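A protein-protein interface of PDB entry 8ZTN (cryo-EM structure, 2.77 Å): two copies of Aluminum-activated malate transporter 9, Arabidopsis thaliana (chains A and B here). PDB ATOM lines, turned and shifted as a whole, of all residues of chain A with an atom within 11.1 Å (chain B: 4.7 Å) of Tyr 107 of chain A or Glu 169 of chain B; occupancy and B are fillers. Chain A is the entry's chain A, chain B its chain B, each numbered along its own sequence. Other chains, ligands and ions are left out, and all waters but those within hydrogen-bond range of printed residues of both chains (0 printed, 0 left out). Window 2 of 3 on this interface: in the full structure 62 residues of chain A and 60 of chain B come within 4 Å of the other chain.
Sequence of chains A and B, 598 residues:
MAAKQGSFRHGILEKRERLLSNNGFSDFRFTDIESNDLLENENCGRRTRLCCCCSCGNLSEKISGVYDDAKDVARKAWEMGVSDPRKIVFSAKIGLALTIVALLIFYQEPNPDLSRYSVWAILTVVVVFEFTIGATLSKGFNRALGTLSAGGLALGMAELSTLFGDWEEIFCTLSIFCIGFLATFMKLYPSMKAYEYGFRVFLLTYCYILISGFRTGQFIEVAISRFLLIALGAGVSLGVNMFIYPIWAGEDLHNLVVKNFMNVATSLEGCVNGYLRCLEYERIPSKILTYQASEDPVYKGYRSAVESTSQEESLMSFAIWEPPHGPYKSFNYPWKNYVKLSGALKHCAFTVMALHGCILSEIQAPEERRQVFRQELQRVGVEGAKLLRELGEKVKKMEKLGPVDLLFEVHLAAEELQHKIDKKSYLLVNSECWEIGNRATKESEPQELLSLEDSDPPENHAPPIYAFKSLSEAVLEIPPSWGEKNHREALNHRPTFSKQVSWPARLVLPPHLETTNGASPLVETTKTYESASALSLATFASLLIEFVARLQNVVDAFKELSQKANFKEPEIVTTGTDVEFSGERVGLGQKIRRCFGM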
ATOM      1  N   LEU A  98      22.864 -29.961  17.812  1.00  0.00           N
ATOM      2  CA  LEU A  98      22.800 -28.514  17.654  1.00  0.00           C
ATOM      3  C   LEU A  98      21.648 -28.115  16.740  1.00  0.00           C
ATOM      4  O   LEU A  98      20.918 -27.160  17.031  1.00  0.00           O
ATOM      5  CB  LEU A  98      24.129 -27.998  17.107  1.00  0.00           C
ATOM      6  CG  LEU A  98      25.123 -27.427  18.122  1.00  0.00           C
ATOM      7  CD1 LEU A  98      26.432 -27.069  17.437  1.00  0.00           C
ATOM      8  CD2 LEU A  98      24.547 -26.235  18.857  1.00  0.00           C
ATOM      9  N   THR A  99      21.461 -28.841  15.634  1.00  0.00           N
ATOM     10  CA  THR A  99      20.361 -28.546  14.723  1.00  0.00           C
ATOM     11  C   THR A  99      19.002 -28.770  15.378  1.00  0.00           C
ATOM     12  O   THR A  99      18.059 -28.014  15.115  1.00  0.00           O
ATOM     13  CB  THR A  99      20.486 -29.397  13.459  1.00  0.00           C
ATOM     14  OG1 THR A  99      21.422 -28.788  12.564  1.00  0.00           O
ATOM     15  CG2 THR A  99      19.142 -29.523  12.765  1.00  0.00           C
ATOM     16  N   ILE A 100      18.883 -29.774  16.249  1.00  0.00           N
ATOM     17  CA  ILE A 100      17.604 -30.003  16.917  1.00  0.00           C
ATOM     18  C   ILE A 100      17.279 -28.841  17.848  1.00  0.00           C
ATOM     19  O   ILE A 100      16.154 -28.320  17.854  1.00  0.00           O
ATOM     20  CB  ILE A 100      17.617 -31.342  17.676  1.00  0.00           C
ATOM     21  CG1 ILE A 100      17.603 -32.519  16.701  1.00  0.00           C
ATOM     22  CG2 ILE A 100      16.436 -31.425  18.628  1.00  0.00           C
ATOM     23  CD1 ILE A 100      17.913 -33.847  17.352  1.00  0.00           C
ATOM     24  N   VAL A 101      18.263 -28.405  18.638  1.00  0.00           N
ATOM     25  CA  VAL A 101      18.006 -27.279  19.535  1.00  0.00           C
ATOM     26  C   VAL A 101      17.706 -26.015  18.734  1.00  0.00           C
ATOM     27  O   VAL A 101      16.833 -25.218  19.104  1.00  0.00           O
ATOM     28  CB  VAL A 101      19.183 -27.077  20.505  1.00  0.00           C
ATOM     29  CG1 VAL A 101      19.066 -25.733  21.195  1.00  0.00           C
ATOM     30  CG2 VAL A 101      19.210 -28.192  21.532  1.00  0.00           C
ATOM     31  N   ALA A 102      18.407 -25.820  17.613  1.00  0.00           N
ATOM     32  CA  ALA A 102      18.178 -24.629  16.803  1.00  0.00           C
ATOM     33  C   ALA A 102      16.774 -24.620  16.216  1.00  0.00           C
ATOM     34  O   ALA A 102      16.116 -23.573  16.178  1.00  0.00           O
ATOM     35  CB  ALA A 102      19.224 -24.540  15.693  1.00  0.00           C
ATOM     36  N   LEU A 103      16.297 -25.772  15.741  1.00  0.00           N
ATOM     37  CA  LEU A 103      14.938 -25.827  15.213  1.00  0.00           C
ATOM     38  C   LEU A 103      13.913 -25.580  16.311  1.00  0.00           C
ATOM     39  O   LEU A 103      12.923 -24.866  16.097  1.00  0.00           O
ATOM     40  CB  LEU A 103      14.685 -27.171  14.535  1.00  0.00           C
ATOM     41  CG  LEU A 103      15.165 -27.302  13.089  1.00  0.00           C
ATOM     42  CD1 LEU A 103      14.817 -28.673  12.534  1.00  0.00           C
ATOM     43  CD2 LEU A 103      14.565 -26.205  12.228  1.00  0.00           C
ATOM     44  N   LEU A 104      14.144 -26.137  17.504  1.00  0.00           N
ATOM     45  CA  LEU A 104      13.206 -25.918  18.599  1.00  0.00           C
ATOM     46  C   LEU A 104      13.211 -24.474  19.077  1.00  0.00           C
ATOM     47  O   LEU A 104      12.219 -24.024  19.660  1.00  0.00           O
ATOM     48  CB  LEU A 104      13.521 -26.848  19.769  1.00  0.00           C
ATOM     49  CG  LEU A 104      12.810 -28.200  19.783  1.00  0.00           C
ATOM     50  CD1 LEU A 104      13.632 -29.224  20.545  1.00  0.00           C
ATOM     51  CD2 LEU A 104      11.425 -28.065  20.386  1.00  0.00           C
ATOM     52  N   ILE A 105      14.297 -23.738  18.840  1.00  0.00           N
ATOM     53  CA  ILE A 105      14.323 -22.332  19.230  1.00  0.00           C
ATOM     54  C   ILE A 105      13.688 -21.458  18.154  1.00  0.00           C
ATOM     55  O   ILE A 105      12.962 -20.508  18.463  1.00  0.00           O
ATOM     56  CB  ILE A 105      15.763 -21.886  19.543  1.00  0.00           C
ATOM     57  CG1 ILE A 105      16.151 -22.288  20.966  1.00  0.00           C
ATOM     58  CG2 ILE A 105      15.911 -20.386  19.346  1.00  0.00           C
ATOM     59  CD1 ILE A 105      17.629 -22.172  21.246  1.00  0.00           C
ATOM     60  N   PHE A 106      13.951 -21.756  16.881  1.00  0.00           N
ATOM     61  CA  PHE A 106      13.345 -20.976  15.806  1.00  0.00           C
ATOM     62  C   PHE A 106      11.831 -21.154  15.766  1.00  0.00           C
ATOM     63  O   PHE A 106      11.095 -20.177  15.586  1.00  0.00           O
ATOM     64  CB  PHE A 106      13.963 -21.353  14.459  1.00  0.00           C
ATOM     65  CG  PHE A 106      15.312 -20.740  14.218  1.00  0.00           C
ATOM     66  CD1 PHE A 106      15.639 -19.515  14.771  1.00  0.00           C
ATOM     67  CD2 PHE A 106      16.253 -21.388  13.438  1.00  0.00           C
ATOM     68  CE1 PHE A 106      16.878 -18.946  14.551  1.00  0.00           C
ATOM     69  CE2 PHE A 106      17.494 -20.825  13.215  1.00  0.00           C
ATOM     70  CZ  PHE A 106      17.807 -19.603  13.773  1.00  0.00           C
ATOM     71  N   TYR A 107      11.344 -22.381  15.932  1.00  0.00           N
ATOM     72  CA  TYR A 107       9.915 -22.675  15.798  1.00  0.00           C
ATOM     73  C   TYR A 107       9.305 -22.896  17.182  1.00  0.00           C
ATOM     74  O   TYR A 107       9.219 -24.026  17.666  1.00  0.00           O
ATOM     75  CB  TYR A 107       9.682 -23.885  14.895  1.00  0.00           C
ATOM     76  CG  TYR A 107      10.239 -23.731  13.498  1.00  0.00           C
ATOM     77  CD1 TYR A 107       9.728 -22.778  12.629  1.00  0.00           C
ATOM     78  CD2 TYR A 107      11.269 -24.543  13.046  1.00  0.00           C
ATOM     79  CE1 TYR A 107      10.231 -22.634  11.351  1.00  0.00           C
ATOM     80  CE2 TYR A 107      11.778 -24.407  11.770  1.00  0.00           C
ATOM     81  CZ  TYR A 107      11.254 -23.452  10.927  1.00  0.00           C
ATOM     82  OH  TYR A 107      11.758 -23.314   9.655  1.00  0.00           O
ATOM     83  N   GLN A 108       8.881 -21.803  17.814  1.00  0.00           N
ATOM     84  CA  GLN A 108       8.198 -21.874  19.099  1.00  0.00           C
ATOM     85  C   GLN A 108       7.261 -20.681  19.217  1.00  0.00           C
ATOM     86  O   GLN A 108       7.408 -19.681  18.510  1.00  0.00           O
ATOM     87  CB  GLN A 108       9.189 -21.907  20.268  1.00  0.00           C
ATOM     88  CG  GLN A 108       9.294 -20.602  21.040  1.00  0.00           C
ATOM     89  CD  GLN A 108      10.145 -19.570  20.328  1.00  0.00           C
ATOM     90  OE1 GLN A 108      10.165 -19.507  19.100  1.00  0.00           O
ATOM     91  NE2 GLN A 108      10.858 -18.759  21.099  1.00  0.00           N
ATOM     92  N   GLU A 109       6.294 -20.796  20.121  1.00  0.00           N
ATOM     93  CA  GLU A 109       5.350 -19.705  20.335  1.00  0.00           C
ATOM     94  C   GLU A 109       6.061 -18.509  20.960  1.00  0.00           C
ATOM     95  O   GLU A 109       6.760 -18.667  21.969  1.00  0.00           O
ATOM     96  CB  GLU A 109       4.199 -20.164  21.226  1.00  0.00           C
ATOM     97  CG  GLU A 109       2.938 -19.324  21.096  1.00  0.00           C
ATOM     98  CD  GLU A 109       3.025 -18.017  21.858  1.00  0.00           C
ATOM     99  OE1 GLU A 109       3.429 -18.042  23.039  1.00  0.00           O
ATOM    100  OE2 GLU A 109       2.690 -16.964  21.275  1.00  0.00           O
ATOM    101  N   PRO A 110       5.909 -17.308  20.404  1.00  0.00           N
ATOM    102  CA  PRO A 110       6.621 -16.149  20.954  1.00  0.00           C
ATOM    103  C   PRO A 110       6.115 -15.775  22.339  1.00  0.00           C
ATOM    104  O   PRO A 110       4.922 -15.876  22.634  1.00  0.00           O
ATOM    105  CB  PRO A 110       6.328 -15.039  19.935  1.00  0.00           C
ATOM    106  CG  PRO A 110       5.057 -15.466  19.274  1.00  0.00           C
ATOM    107  CD  PRO A 110       5.125 -16.962  19.207  1.00  0.00           C
ATOM    108  N   ASN A 111       7.039 -15.336  23.191  1.00  0.00           N
ATOM    109  CA  ASN A 111       6.715 -14.883  24.536  1.00  0.00           C
ATOM    110  C   ASN A 111       7.814 -13.909  24.934  1.00  0.00           C
ATOM    111  O   ASN A 111       8.951 -14.041  24.467  1.00  0.00           O
ATOM    112  CB  ASN A 111       6.601 -16.087  25.499  1.00  0.00           C
ATOM    113  CG  ASN A 111       6.890 -15.754  26.971  1.00  0.00           C
ATOM    114  OD1 ASN A 111       6.744 -14.632  27.426  1.00  0.00           O
ATOM    115  ND2 ASN A 111       7.251 -16.775  27.730  1.00  0.00           N
ATOM    116  N   LEU A 114      11.139 -15.604  27.162  1.00  0.00           N
ATOM    117  CA  LEU A 114      11.967 -16.562  26.428  1.00  0.00           C
ATOM    118  C   LEU A 114      12.840 -15.867  25.390  1.00  0.00           C
ATOM    119  O   LEU A 114      14.024 -16.190  25.249  1.00  0.00           O
ATOM    120  CB  LEU A 114      11.125 -17.649  25.759  1.00  0.00           C
ATOM    121  CG  LEU A 114      10.529 -18.772  26.613  1.00  0.00           C
ATOM    122  CD1 LEU A 114       9.040 -18.636  26.764  1.00  0.00           C
ATOM    123  CD2 LEU A 114      10.882 -20.129  26.018  1.00  0.00           C
ATOM    124  N   SER A 118      16.602 -17.403  25.452  1.00  0.00           N
ATOM    125  CA  SER A 118      16.421 -18.683  24.782  1.00  0.00           C
ATOM    126  C   SER A 118      17.708 -19.206  24.165  1.00  0.00           C
ATOM    127  O   SER A 118      17.757 -20.375  23.768  1.00  0.00           O
ATOM    128  CB  SER A 118      15.341 -18.571  23.702  1.00  0.00           C
ATOM    129  OG  SER A 118      15.739 -17.674  22.681  1.00  0.00           O
ATOM    130  N   ILE A 122      21.237 -23.595  23.404  1.00  0.00           N
ATOM    131  CA  ILE A 122      22.173 -24.021  22.364  1.00  0.00           C
ATOM    132  C   ILE A 122      23.622 -23.895  22.797  1.00  0.00           C
ATOM    133  O   ILE A 122      24.507 -24.443  22.129  1.00  0.00           O
ATOM    134  CB  ILE A 122      21.959 -23.226  21.063  1.00  0.00           C
ATOM    135  CG1 ILE A 122      22.751 -23.855  19.916  1.00  0.00           C
ATOM    136  CG2 ILE A 122      22.357 -21.773  21.250  1.00  0.00           C
ATOM    137  CD1 ILE A 122      22.005 -23.899  18.605  1.00  0.00           C
ATOM    138  N   LEU A 232      17.200 -28.564  29.649  1.00  0.00           N
ATOM    139  CA  LEU A 232      16.749 -29.066  28.353  1.00  0.00           C
ATOM    140  C   LEU A 232      17.916 -29.293  27.397  1.00  0.00           C
ATOM    141  O   LEU A 232      17.944 -30.299  26.668  1.00  0.00           O
ATOM    142  CB  LEU A 232      15.739 -28.094  27.745  1.00  0.00           C
ATOM    143  CG  LEU A 232      15.214 -28.413  26.345  1.00  0.00           C
ATOM    144  CD1 LEU A 232      13.938 -29.236  26.426  1.00  0.00           C
ATOM    145  CD2 LEU A 232      14.980 -27.136  25.557  1.00  0.00           C
ATOM    146  N   TRP B 167      13.127 -19.302   2.466  1.00  0.00           N
ATOM    147  CA  TRP B 167      13.617 -20.163   3.542  1.00  0.00           C
ATOM    148  C   TRP B 167      14.858 -19.532   4.166  1.00  0.00           C
ATOM    149  O   TRP B 167      15.990 -19.911   3.860  1.00  0.00           O
ATOM    150  CB  TRP B 167      13.905 -21.578   3.018  1.00  0.00           C
ATOM    151  CG  TRP B 167      12.965 -22.028   1.943  1.00  0.00           C
ATOM    152  CD1 TRP B 167      11.603 -22.053   2.004  1.00  0.00           C
ATOM    153  CD2 TRP B 167      13.317 -22.531   0.649  1.00  0.00           C
ATOM    154  NE1 TRP B 167      11.084 -22.534   0.826  1.00  0.00           N
ATOM    155  CE2 TRP B 167      12.116 -22.836  -0.021  1.00  0.00           C
ATOM    156  CE3 TRP B 167      14.532 -22.752  -0.009  1.00  0.00           C
ATOM    157  CZ2 TRP B 167      12.094 -23.349  -1.316  1.00  0.00           C
ATOM    158  CZ3 TRP B 167      14.507 -23.261  -1.294  1.00  0.00           C
ATOM    159  CH2 TRP B 167      13.297 -23.553  -1.934  1.00  0.00           C
ATOM    160  N   GLU B 168      14.636 -18.561   5.055  1.00  0.00           N
ATOM    161  CA  GLU B 168      15.737 -17.951   5.791  1.00  0.00           C
ATOM    162  C   GLU B 168      16.163 -18.833   6.958  1.00  0.00           C
ATOM    163  O   GLU B 168      17.351 -19.146   7.119  1.00  0.00           O
ATOM    164  CB  GLU B 168      15.329 -16.563   6.290  1.00  0.00           C
ATOM    165  CG  GLU B 168      16.497 -15.640   6.591  1.00  0.00           C
ATOM    166  CD  GLU B 168      16.702 -14.589   5.519  1.00  0.00           C
ATOM    167  OE1 GLU B 168      16.175 -14.769   4.401  1.00  0.00           O
ATOM    168  OE2 GLU B 168      17.388 -13.584   5.796  1.00  0.00           O
ATOM    169  N   GLU B 169      15.194 -19.255   7.773  1.00  0.00           N
ATOM    170  CA  GLU B 169      15.504 -20.052   8.950  1.00  0.00           C
ATOM    171  C   GLU B 169      16.041 -21.423   8.569  1.00  0.00           C
ATOM    172  O   GLU B 169      16.850 -21.990   9.306  1.00  0.00           O
ATOM    173  CB  GLU B 169      14.263 -20.192   9.830  1.00  0.00           C
ATOM    174  CG  GLU B 169      13.003 -20.561   9.069  1.00  0.00           C
ATOM    175  CD  GLU B 169      12.224 -19.346   8.608  1.00  0.00           C
ATOM    176  OE1 GLU B 169      12.846 -18.286   8.396  1.00  0.00           O
ATOM    177  OE2 GLU B 169      10.988 -19.453   8.457  1.00  0.00           O
ATOM    178  N   ILE B 170      15.634 -21.958   7.417  1.00  0.00           N
ATOM    179  CA  ILE B 170      16.155 -23.251   6.988  1.00  0.00           C
ATOM    180  C   ILE B 170      17.646 -23.148   6.689  1.00  0.00           C
ATOM    181  O   ILE B 170      18.442 -23.986   7.122  1.00  0.00           O
ATOM    182  CB  ILE B 170      15.371 -23.771   5.770  1.00  0.00           C
ATOM    183  CG1 ILE B 170      13.907 -24.012   6.142  1.00  0.00           C
ATOM    184  CG2 ILE B 170      16.006 -25.042   5.231  1.00  0.00           C
ATOM    185  CD1 ILE B 170      13.724 -24.778   7.431  1.00  0.00           C
ATOM    186  N   PHE B 171      18.050 -22.105   5.962  1.00  0.00           N
ATOM    187  CA  PHE B 171      19.466 -21.918   5.657  1.00  0.00           C
ATOM    188  C   PHE B 171      20.263 -21.616   6.924  1.00  0.00           C
ATOM    189  O   PHE B 171      21.377 -22.137   7.114  1.00  0.00           O
ATOM    190  CB  PHE B 171      19.612 -20.802   4.619  1.00  0.00           C
ATOM    191  CG  PHE B 171      21.016 -20.298   4.441  1.00  0.00           C
ATOM    192  CD1 PHE B 171      21.892 -20.941   3.585  1.00  0.00           C
ATOM    193  CD2 PHE B 171      21.448 -19.161   5.101  1.00  0.00           C
ATOM    194  CE1 PHE B 171      23.178 -20.473   3.408  1.00  0.00           C
ATOM    195  CE2 PHE B 171      22.733 -18.689   4.928  1.00  0.00           C
ATOM    196  CZ  PHE B 171      23.599 -19.346   4.080  1.00  0.00           C
ATOM    197  N   CYS B 172      19.682 -20.832   7.835  1.00  0.00           N
ATOM    198  CA  CYS B 172      20.407 -20.504   9.056  1.00  0.00           C
ATOM    199  C   CYS B 172      20.573 -21.732   9.941  1.00  0.00           C
ATOM    200  O   CYS B 172      21.624 -21.911  10.568  1.00  0.00           O
ATOM    201  CB  CYS B 172      19.688 -19.387   9.809  1.00  0.00           C
ATOM    202  SG  CYS B 172      20.044 -17.730   9.184  1.00  0.00           S
ATOM    203  N   THR B 173      19.556 -22.593  10.006  1.00  0.00           N
ATOM    204  CA  THR B 173      19.678 -23.836  10.753  1.00  0.00           C
ATOM    205  C   THR B 173      20.466 -24.894   9.997  1.00  0.00           C
ATOM    206  O   THR B 173      20.839 -25.908  10.597  1.00  0.00           O
ATOM    207  CB  THR B 173      18.291 -24.381  11.104  1.00  0.00           C
ATOM    208  OG1 THR B 173      18.409 -25.365  12.138  1.00  0.00           O
ATOM    209  CG2 THR B 173      17.648 -25.015   9.884  1.00  0.00           C
ATOM    210  N   PHE B 214      18.687 -12.940  14.870  1.00  0.00           N
ATOM    211  CA  PHE B 214      17.564 -13.296  14.006  1.00  0.00           C
ATOM    212  C   PHE B 214      16.360 -12.403  14.275  1.00  0.00           C
ATOM    213  O   PHE B 214      15.684 -11.963  13.338  1.00  0.00           O
ATOM    214  CB  PHE B 214      17.196 -14.765  14.208  1.00  0.00           C
ATOM    215  CG  PHE B 214      16.228 -15.294  13.191  1.00  0.00           C
ATOM    216  CD1 PHE B 214      16.604 -15.444  11.869  1.00  0.00           C
ATOM    217  CD2 PHE B 214      14.940 -15.645  13.562  1.00  0.00           C
ATOM    218  CE1 PHE B 214      15.714 -15.932  10.932  1.00  0.00           C
ATOM    219  CE2 PHE B 214      14.046 -16.134  12.630  1.00  0.00           C
ATOM    220  CZ  PHE B 214      14.433 -16.278  11.314  1.00  0.00           C
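No position is printed for both chains. Of the 6 pairs that touch across the chains among the printed residues, none has its exchanged pair printed and touching as well.
Printed residues of chain B within 4 Å of Thr 99 of chain A: Thr 173 (3.5 Å). Printed residues of chain B within 4 Å of Ala 102 of chain A: Thr 173. Printed residues of chain B within 4 Å of Leu 103 of chain A: Thr 173 (3.9 Å). Asn 111 of chain A touches none of the printed residues of chain B. No residue of chain A comes within 4 Å of Glu 168 of chain B. Of the printed residues of chain A, Glu 169 of chain B touches Tyr 107. Cys 172 of chain B touches none of the printed residues of chain A. Printed residues of chain A within 4 Å of Thr 173 of chain B: Thr 99 (3.5 Å), Ala 102 (3.7 Å) and Leu 103 (3.9 Å). Printed residues of chain A within 4 Å of Phe 214 of chain B: Phe 106. The nearest printed residue of chain B that does not touch Tyr 107 of chain A is Thr 173 of chain B (6.1 Å).
Printed residues of chain A that touch a printed residue of chain B: Thr 99, Ala 102, Leu 103, Phe 106 and Tyr 107. Among the printed residues, 6 pairs touch across the chains.
Among the printed residues, merely in contact across the chains: Tyr 107 of chain A with Glu 169 of chain B (3.1 Å), Tyr 107 of chain A with Ile 170 of chain B (3.3 Å), Thr 99 of chain A with Thr 173 of chain B (3.5 Å), Ala 102 of chain A with Thr 173 of chain B (3.7 Å), Leu 103 of chain A with Thr 173 of chain B (3.9 Å) and Phe 106 of chain A with Phe 214 of chain B (3.95 Å).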
